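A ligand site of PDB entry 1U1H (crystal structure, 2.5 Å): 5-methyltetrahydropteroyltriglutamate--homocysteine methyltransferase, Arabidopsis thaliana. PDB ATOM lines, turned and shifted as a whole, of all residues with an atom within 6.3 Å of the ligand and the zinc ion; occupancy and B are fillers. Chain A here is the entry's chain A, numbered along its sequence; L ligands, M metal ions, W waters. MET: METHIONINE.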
ATOM      1  N   ILE A 437      -2.059   5.580  24.856  1.00  0.00           N
ATOM      2  CA  ILE A 437      -2.914   5.369  23.701  1.00  0.00           C
ATOM      3  C   ILE A 437      -2.237   5.181  22.340  1.00  0.00           C
ATOM      4  O   ILE A 437      -2.879   4.721  21.400  1.00  0.00           O
ATOM      5  CB  ILE A 437      -3.943   6.480  23.599  1.00  0.00           C
ATOM      6  CG1 ILE A 437      -4.663   6.622  24.940  1.00  0.00           C
ATOM      7  CG2 ILE A 437      -4.956   6.172  22.505  1.00  0.00           C
ATOM      8  CD1 ILE A 437      -5.240   5.328  25.464  1.00  0.00           C
ATOM      9  N   GLY A 438      -0.956   5.521  22.226  1.00  0.00           N
ATOM     10  CA  GLY A 438      -0.297   5.318  20.950  1.00  0.00           C
ATOM     11  C   GLY A 438       0.871   6.199  20.560  1.00  0.00           C
ATOM     12  O   GLY A 438       2.031   5.797  20.664  1.00  0.00           O
ATOM     13  N   SER A 439       0.569   7.410  20.104  1.00  0.00           N
ATOM     14  CA  SER A 439       1.609   8.334  19.680  1.00  0.00           C
ATOM     15  C   SER A 439       2.337   9.039  20.815  1.00  0.00           C
ATOM     16  O   SER A 439       1.802   9.207  21.918  1.00  0.00           O
ATOM     17  CB  SER A 439       0.995   9.391  18.746  1.00  0.00           C
ATOM     18  OG  SER A 439      -0.018  10.134  19.416  1.00  0.00           O
ATOM     19  N   PHE A 440       3.565   9.446  20.517  1.00  0.00           N
ATOM     20  CA  PHE A 440       4.417  10.187  21.452  1.00  0.00           C
ATOM     21  C   PHE A 440       4.912  11.446  20.742  1.00  0.00           C
ATOM     22  O   PHE A 440       4.988  11.475  19.515  1.00  0.00           O
ATOM     23  CB  PHE A 440       5.611   9.339  21.911  1.00  0.00           C
ATOM     24  CG  PHE A 440       5.404   8.674  23.244  1.00  0.00           C
ATOM     25  CD1 PHE A 440       4.510   7.611  23.376  1.00  0.00           C
ATOM     26  CD2 PHE A 440       6.078   9.115  24.372  1.00  0.00           C
ATOM     27  CE1 PHE A 440       4.289   7.006  24.619  1.00  0.00           C
ATOM     28  CE2 PHE A 440       5.868   8.513  25.624  1.00  0.00           C
ATOM     29  CZ  PHE A 440       4.964   7.462  25.740  1.00  0.00           C
ATOM     30  N   GLU A 490       4.431   5.396  17.217  1.00  0.00           N
ATOM     31  CA  GLU A 490       4.005   5.645  15.829  1.00  0.00           C
ATOM     32  C   GLU A 490       4.853   6.698  15.109  1.00  0.00           C
ATOM     33  O   GLU A 490       4.329   7.457  14.273  1.00  0.00           O
ATOM     34  CB  GLU A 490       2.545   6.093  15.795  1.00  0.00           C
ATOM     35  CG  GLU A 490       1.539   5.077  16.298  1.00  0.00           C
ATOM     36  CD  GLU A 490       0.205   5.721  16.638  1.00  0.00           C
ATOM     37  OE1 GLU A 490      -0.330   6.477  15.794  1.00  0.00           O
ATOM     38  OE2 GLU A 490      -0.309   5.481  17.751  1.00  0.00           O
ATOM     39  N   ARG A 493       4.354   7.128  11.283  1.00  0.00           N
ATOM     40  CA  ARG A 493       3.028   7.454  10.743  1.00  0.00           C
ATOM     41  C   ARG A 493       2.724   8.947  10.783  1.00  0.00           C
ATOM     42  O   ARG A 493       2.908   9.603  11.819  1.00  0.00           O
ATOM     43  CB  ARG A 493       1.952   6.696  11.512  1.00  0.00           C
ATOM     44  CG  ARG A 493       2.202   5.215  11.624  1.00  0.00           C
ATOM     45  CD  ARG A 493       1.135   4.527  12.457  1.00  0.00           C
ATOM     46  NE  ARG A 493       1.468   3.122  12.678  1.00  0.00           N
ATOM     47  CZ  ARG A 493       0.676   2.259  13.306  1.00  0.00           C
ATOM     48  NH1 ARG A 493      -0.497   2.665  13.771  1.00  0.00           N
ATOM     49  NH2 ARG A 493       1.058   1.005  13.462  1.00  0.00           N
ATOM     50  N   MET A 496      -3.387   8.887  10.916  1.00  0.00           N
ATOM     51  CA  MET A 496      -4.120   7.682  11.327  1.00  0.00           C
ATOM     52  C   MET A 496      -4.664   6.878  10.170  1.00  0.00           C
ATOM     53  O   MET A 496      -4.501   5.663  10.103  1.00  0.00           O
ATOM     54  CB  MET A 496      -5.328   8.058  12.171  1.00  0.00           C
ATOM     55  CG  MET A 496      -5.130   8.166  13.642  1.00  0.00           C
ATOM     56  SD  MET A 496      -6.883   8.574  14.329  1.00  0.00           S
ATOM     57  CE  MET A 496      -7.575   6.782  14.627  1.00  0.00           C
ATOM     58  N   MET A 557      -0.827  -1.374  16.704  1.00  0.00           N
ATOM     59  CA  MET A 557      -1.635  -0.201  16.467  1.00  0.00           C
ATOM     60  C   MET A 557      -2.317  -0.160  15.111  1.00  0.00           C
ATOM     61  O   MET A 557      -1.670  -0.034  14.070  1.00  0.00           O
ATOM     62  CB  MET A 557      -0.778   1.061  16.655  1.00  0.00           C
ATOM     63  CG  MET A 557      -0.640   1.509  18.102  1.00  0.00           C
ATOM     64  SD  MET A 557      -2.347   2.066  18.797  1.00  0.00           S
ATOM     65  CE  MET A 557      -2.909   3.076  17.276  1.00  0.00           C
ATOM     66  N   TRP A 567     -13.667   9.060   7.675  1.00  0.00           N
ATOM     67  CA  TRP A 567     -12.766  10.147   7.306  1.00  0.00           C
ATOM     68  C   TRP A 567     -12.166  10.048   5.908  1.00  0.00           C
ATOM     69  O   TRP A 567     -11.056  10.530   5.642  1.00  0.00           O
ATOM     70  CB  TRP A 567     -11.671  10.292   8.380  1.00  0.00           C
ATOM     71  CG  TRP A 567     -12.213  10.830   9.682  1.00  0.00           C
ATOM     72  CD1 TRP A 567     -13.428  11.453   9.875  1.00  0.00           C
ATOM     73  CD2 TRP A 567     -11.564  10.845  10.964  1.00  0.00           C
ATOM     74  NE1 TRP A 567     -13.569  11.845  11.189  1.00  0.00           N
ATOM     75  CE2 TRP A 567     -12.434  11.485  11.873  1.00  0.00           C
ATOM     76  CE3 TRP A 567     -10.327  10.368  11.422  1.00  0.00           C
ATOM     77  CZ2 TRP A 567     -12.107  11.667  13.222  1.00  0.00           C
ATOM     78  CZ3 TRP A 567     -10.007  10.561  12.765  1.00  0.00           C
ATOM     79  CH2 TRP A 567     -10.893  11.201  13.646  1.00  0.00           C
ATOM     80  N   GLN A 603      -4.083  -3.121  19.645  1.00  0.00           N
ATOM     81  CA  GLN A 603      -5.016  -2.015  19.843  1.00  0.00           C
ATOM     82  C   GLN A 603      -5.619  -1.544  18.520  1.00  0.00           C
ATOM     83  O   GLN A 603      -4.917  -1.309  17.550  1.00  0.00           O
ATOM     84  CB  GLN A 603      -4.320  -0.845  20.533  1.00  0.00           C
ATOM     85  CG  GLN A 603      -5.255   0.278  20.924  1.00  0.00           C
ATOM     86  CD  GLN A 603      -4.585   1.318  21.804  1.00  0.00           C
ATOM     87  OE1 GLN A 603      -4.077   1.005  22.887  1.00  0.00           O
ATOM     88  NE2 GLN A 603      -4.581   2.560  21.354  1.00  0.00           N
ATOM     89  N   ASP A 605      -8.049   1.453  17.322  1.00  0.00           N
ATOM     90  CA  ASP A 605      -8.795   2.640  17.732  1.00  0.00           C
ATOM     91  C   ASP A 605      -9.822   3.088  16.704  1.00  0.00           C
ATOM     92  O   ASP A 605      -9.534   3.203  15.507  1.00  0.00           O
ATOM     93  CB  ASP A 605      -7.833   3.788  18.081  1.00  0.00           C
ATOM     94  CG  ASP A 605      -6.729   3.974  17.058  1.00  0.00           C
ATOM     95  OD1 ASP A 605      -7.022   3.836  15.856  1.00  0.00           O
ATOM     96  OD2 ASP A 605      -5.571   4.273  17.446  1.00  0.00           O
ATOM     97  N   GLU A 606     -11.044   3.299  17.185  1.00  0.00           N
ATOM     98  CA  GLU A 606     -12.149   3.752  16.355  1.00  0.00           C
ATOM     99  C   GLU A 606     -12.461   5.167  16.821  1.00  0.00           C
ATOM    100  O   GLU A 606     -13.485   5.429  17.442  1.00  0.00           O
ATOM    101  CB  GLU A 606     -13.359   2.845  16.531  1.00  0.00           C
ATOM    102  CG  GLU A 606     -13.253   1.544  15.749  1.00  0.00           C
ATOM    103  CD  GLU A 606     -13.391   1.777  14.257  1.00  0.00           C
ATOM    104  OE1 GLU A 606     -12.853   2.791  13.761  1.00  0.00           O
ATOM    105  OE2 GLU A 606     -14.015   0.955  13.577  1.00  0.00           O
ATOM    106  N   ALA A 607     -11.538   6.066  16.503  1.00  0.00           N
ATOM    107  CA  ALA A 607     -11.634   7.466  16.873  1.00  0.00           C
ATOM    108  C   ALA A 607     -12.914   8.110  16.384  1.00  0.00           C
ATOM    109  O   ALA A 607     -13.420   9.043  17.001  1.00  0.00           O
ATOM    110  CB  ALA A 607     -10.433   8.232  16.306  1.00  0.00           C
ATOM    111  N   HIS A 647      -9.751   1.882  21.141  1.00  0.00           N
ATOM    112  CA  HIS A 647      -9.728   3.238  21.672  1.00  0.00           C
ATOM    113  C   HIS A 647     -10.797   4.116  21.001  1.00  0.00           C
ATOM    114  O   HIS A 647     -10.966   4.061  19.785  1.00  0.00           O
ATOM    115  CB  HIS A 647      -8.350   3.854  21.473  1.00  0.00           C
ATOM    116  CG  HIS A 647      -8.288   5.305  21.836  1.00  0.00           C
ATOM    117  ND1 HIS A 647      -8.565   5.765  23.101  1.00  0.00           N
ATOM    118  CD2 HIS A 647      -8.039   6.401  21.079  1.00  0.00           C
ATOM    119  CE1 HIS A 647      -8.476   7.083  23.117  1.00  0.00           C
ATOM    120  NE2 HIS A 647      -8.157   7.492  21.907  1.00  0.00           N
ATOM    121  N   MET A 648     -11.495   4.931  21.787  1.00  0.00           N
ATOM    122  CA  MET A 648     -12.538   5.808  21.235  1.00  0.00           C
ATOM    123  C   MET A 648     -12.544   7.216  21.815  1.00  0.00           C
ATOM    124  O   MET A 648     -12.804   7.420  22.995  1.00  0.00           O
ATOM    125  CB  MET A 648     -13.914   5.171  21.430  1.00  0.00           C
ATOM    126  CG  MET A 648     -14.076   3.861  20.689  1.00  0.00           C
ATOM    127  SD  MET A 648     -15.702   2.953  21.142  1.00  0.00           S
ATOM    128  CE  MET A 648     -15.165   2.286  22.872  1.00  0.00           C
ATOM    129  N   CYS A 649     -12.288   8.193  20.950  1.00  0.00           N
ATOM    130  CA  CYS A 649     -12.249   9.593  21.350  1.00  0.00           C
ATOM    131  C   CYS A 649     -13.605  10.170  21.735  1.00  0.00           C
ATOM    132  O   CYS A 649     -14.127  11.020  21.031  1.00  0.00           O
ATOM    133  CB  CYS A 649     -11.640  10.414  20.223  1.00  0.00           C
ATOM    134  SG  CYS A 649     -10.175   9.670  19.486  1.00  0.00           S
ATOM    135  N   TYR A 650     -14.163   9.726  22.860  1.00  0.00           N
ATOM    136  CA  TYR A 650     -15.464  10.214  23.319  1.00  0.00           C
ATOM    137  C   TYR A 650     -15.576  10.072  24.846  1.00  0.00           C
ATOM    138  O   TYR A 650     -14.857   9.292  25.453  1.00  0.00           O
ATOM    139  CB  TYR A 650     -16.598   9.403  22.678  1.00  0.00           C
ATOM    140  CG  TYR A 650     -16.630   9.438  21.165  1.00  0.00           C
ATOM    141  CD1 TYR A 650     -17.055  10.579  20.474  1.00  0.00           C
ATOM    142  CD2 TYR A 650     -16.248   8.325  20.417  1.00  0.00           C
ATOM    143  CE1 TYR A 650     -17.100  10.599  19.087  1.00  0.00           C
ATOM    144  CE2 TYR A 650     -16.296   8.332  19.027  1.00  0.00           C
ATOM    145  CZ  TYR A 650     -16.719   9.475  18.368  1.00  0.00           C
ATOM    146  OH  TYR A 650     -16.789   9.479  16.983  1.00  0.00           O
ATOM    147  N   GLU A 671     -12.427   8.620  26.582  1.00  0.00           N
ATOM    148  CA  GLU A 671     -12.045   9.952  27.054  1.00  0.00           C
ATOM    149  C   GLU A 671     -12.693  10.223  28.403  1.00  0.00           C
ATOM    150  O   GLU A 671     -13.880   9.953  28.593  1.00  0.00           O
ATOM    151  CB  GLU A 671     -12.485  11.013  26.069  1.00  0.00           C
ATOM    152  CG  GLU A 671     -11.450  11.335  25.026  1.00  0.00           C
ATOM    153  CD  GLU A 671     -11.932  12.368  24.045  1.00  0.00           C
ATOM    154  OE1 GLU A 671     -12.620  13.309  24.487  1.00  0.00           O
ATOM    155  OE2 GLU A 671     -11.599  12.251  22.854  1.00  0.00           O
ATOM    156  N   ILE A 700      -4.811  15.386  27.335  1.00  0.00           N
ATOM    157  CA  ILE A 700      -3.714  15.633  26.409  1.00  0.00           C
ATOM    158  C   ILE A 700      -3.856  16.904  25.571  1.00  0.00           C
ATOM    159  O   ILE A 700      -2.965  17.251  24.797  1.00  0.00           O
ATOM    160  CB  ILE A 700      -3.542  14.471  25.419  1.00  0.00           C
ATOM    161  CG1 ILE A 700      -4.821  14.298  24.592  1.00  0.00           C
ATOM    162  CG2 ILE A 700      -3.200  13.194  26.176  1.00  0.00           C
ATOM    163  CD1 ILE A 700      -4.572  13.836  23.176  1.00  0.00           C
ATOM    164  N   ASP A 732      -5.925  10.479  28.078  1.00  0.00           N
ATOM    165  CA  ASP A 732      -7.158  10.759  27.339  1.00  0.00           C
ATOM    166  C   ASP A 732      -7.061  10.339  25.884  1.00  0.00           C
ATOM    167  O   ASP A 732      -8.052   9.952  25.271  1.00  0.00           O
ATOM    168  CB  ASP A 732      -7.477  12.258  27.373  1.00  0.00           C
ATOM    169  CG  ASP A 732      -8.557  12.612  28.371  1.00  0.00           C
ATOM    170  OD1 ASP A 732      -9.209  11.687  28.901  1.00  0.00           O
ATOM    171  OD2 ASP A 732      -8.771  13.824  28.606  1.00  0.00           O
ATOM    172  N   CYS A 733      -5.858  10.452  25.325  1.00  0.00           N
ATOM    173  CA  CYS A 733      -5.611  10.089  23.939  1.00  0.00           C
ATOM    174  C   CYS A 733      -4.114  10.046  23.687  1.00  0.00           C
ATOM    175  O   CYS A 733      -3.329   9.966  24.635  1.00  0.00           O
ATOM    176  CB  CYS A 733      -6.266  11.099  22.995  1.00  0.00           C
ATOM    177  SG  CYS A 733      -6.301  10.574  21.247  1.00  0.00           S
ATOM    178  N   GLY A 734      -3.730  10.097  22.422  1.00  0.00           N
ATOM    179  CA  GLY A 734      -2.317  10.069  22.047  1.00  0.00           C
ATOM    180  C   GLY A 734      -1.577  11.261  22.615  1.00  0.00           C
ATOM    181  O   GLY A 734      -2.184  12.145  23.226  1.00  0.00           O
ATOM    182  N   LEU A 735      -0.262  11.299  22.402  1.00  0.00           N
ATOM    183  CA  LEU A 735       0.566  12.384  22.907  1.00  0.00           C
ATOM    184  C   LEU A 735       1.265  13.182  21.797  1.00  0.00           C
ATOM    185  O   LEU A 735       2.084  14.060  22.065  1.00  0.00           O
ATOM    186  CB  LEU A 735       1.609  11.829  23.879  1.00  0.00           C
ATOM    187  CG  LEU A 735       1.065  11.090  25.100  1.00  0.00           C
ATOM    188  CD1 LEU A 735       2.236  10.535  25.915  1.00  0.00           C
ATOM    189  CD2 LEU A 735       0.190  12.018  25.951  1.00  0.00           C
ATOM    190  N   LYS A 736       0.931  12.862  20.548  1.00  0.00           N
ATOM    191  CA  LYS A 736       1.517  13.511  19.383  1.00  0.00           C
ATOM    192  C   LYS A 736       1.622  15.038  19.499  1.00  0.00           C
ATOM    193  O   LYS A 736       2.684  15.615  19.263  1.00  0.00           O
ATOM    194  CB  LYS A 736       0.680  13.136  18.160  1.00  0.00           C
ATOM    195  CG  LYS A 736       1.290  13.426  16.794  1.00  0.00           C
ATOM    196  CD  LYS A 736       0.363  12.864  15.702  1.00  0.00           C
ATOM    197  CE  LYS A 736       0.963  12.947  14.309  1.00  0.00           C
ATOM    198  NZ  LYS A 736       0.160  12.144  13.319  1.00  0.00           N
HETATM  199  N   MET L   1      -3.236   5.576  18.491  1.00  0.00           N
HETATM  200  CA  MET L   1      -3.208   6.937  17.881  1.00  0.00           C
HETATM  201  C   MET L   1      -2.587   7.940  18.850  1.00  0.00           C
HETATM  202  O   MET L   1      -2.226   7.545  19.973  1.00  0.00           O
HETATM  203  CB  MET L   1      -4.626   7.376  17.522  1.00  0.00           C
HETATM  204  CG  MET L   1      -5.495   7.735  18.711  1.00  0.00           C
HETATM  205  SD  MET L   1      -7.204   8.104  18.239  1.00  0.00           S
HETATM  206  CE  MET L   1      -7.067   9.779  17.560  1.00  0.00           C
HETATM  207  OXT MET L   1      -2.475   9.119  18.456  1.00  0.00           O
HETATM  208 ZN    ZN M   1      -8.522   9.544  21.254  1.00  0.00          ZN
HETATM  209  O   HOH W   1      -9.609  10.290  23.135  1.00  0.00           O
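N of Glu 606 lies within hydrogen-bond range of O of His 647 (2.7 Å). NE2 of Gln 603 is in hydrogen-bond range of SD of Met 557 (3.4 Å). The backbone carbonyl oxygen (O) of Met 557 sits at hydrogen-bond distance from the guanidinium group (NH1) of Arg 493 (3.0 Å). The backbone NH (N) of Ser 439 lies within hydrogen-bond range of the side-chain carboxylate (OE2) of Glu 490 (3.2 Å). The backbone carbonyl oxygen of Ser 439 lies within hydrogen-bond range of the backbone NH of Leu 735, at 3.0 Å. The side-chain hydroxyl of Ser 439 is in hydrogen-bond range of the backbone NH of Lys 736 (3.1 Å). The backbone carbonyl oxygen of Ile 437 lies within hydrogen-bond range of the side-chain amide nitrogen of Gln 603, 2.8 Å away. O of Ala 607 is in hydrogen-bond range of OH of Tyr 650, 3.4 Å away.
The side-chain sulfur (SG) of Cys 649 lies close to a sulfur (SD) of the ligand. The side-chain sulfur of Met 557 lies close to a nitrogen (N) of the ligand (3.6 Å). N of Ser 439 lies within hydrogen-bond range of O of the ligand, at 2.8 Å. The side-chain hydroxyl (OG) of Ser 439 sits at hydrogen-bond distance from an oxygen (OXT) of the ligand (2.8 Å). The side-chain carboxylate of Asp 605 lies within salt-bridge range of a nitrogen (N) of the ligand (2.9 Å). A nitrogen (N) of the ligand is in salt-bridge range of the side-chain carboxylate (OE2) of Glu 490. O of Ile 437 sits at hydrogen-bond distance from N of the ligand (3.1 Å). N of Gly 438 sits close to O of the ligand (3.3 Å).
Water W1 lies within hydrogen-bond range of the backbone carbonyl oxygen (O) of Asp 732 and the side-chain carboxylate (OE2) of Glu 671.
Met 496 touches the ligand (SD to CE, 3.5 Å). Ala 607 touches the ligand (CB to SD, 3.8 Å). Gly 734 touches the ligand. Hydrophobic or aromatic side chains that line the ligand: Ile 437, Met 496, Met 557, Ala 607 and His 647.
Within 4 Å of the zinc ion: His 647, Cys 649 and Cys 733.
The zinc ion is bound by NE2 of His 647, 2.2 Å away. The zinc ion is bound by water W1, at 2.3 Å. The zinc ion is bound by SG of Cys 649, 2.4 Å away. SG of Cys 733 binds the zinc ion, at 2.4 Å.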
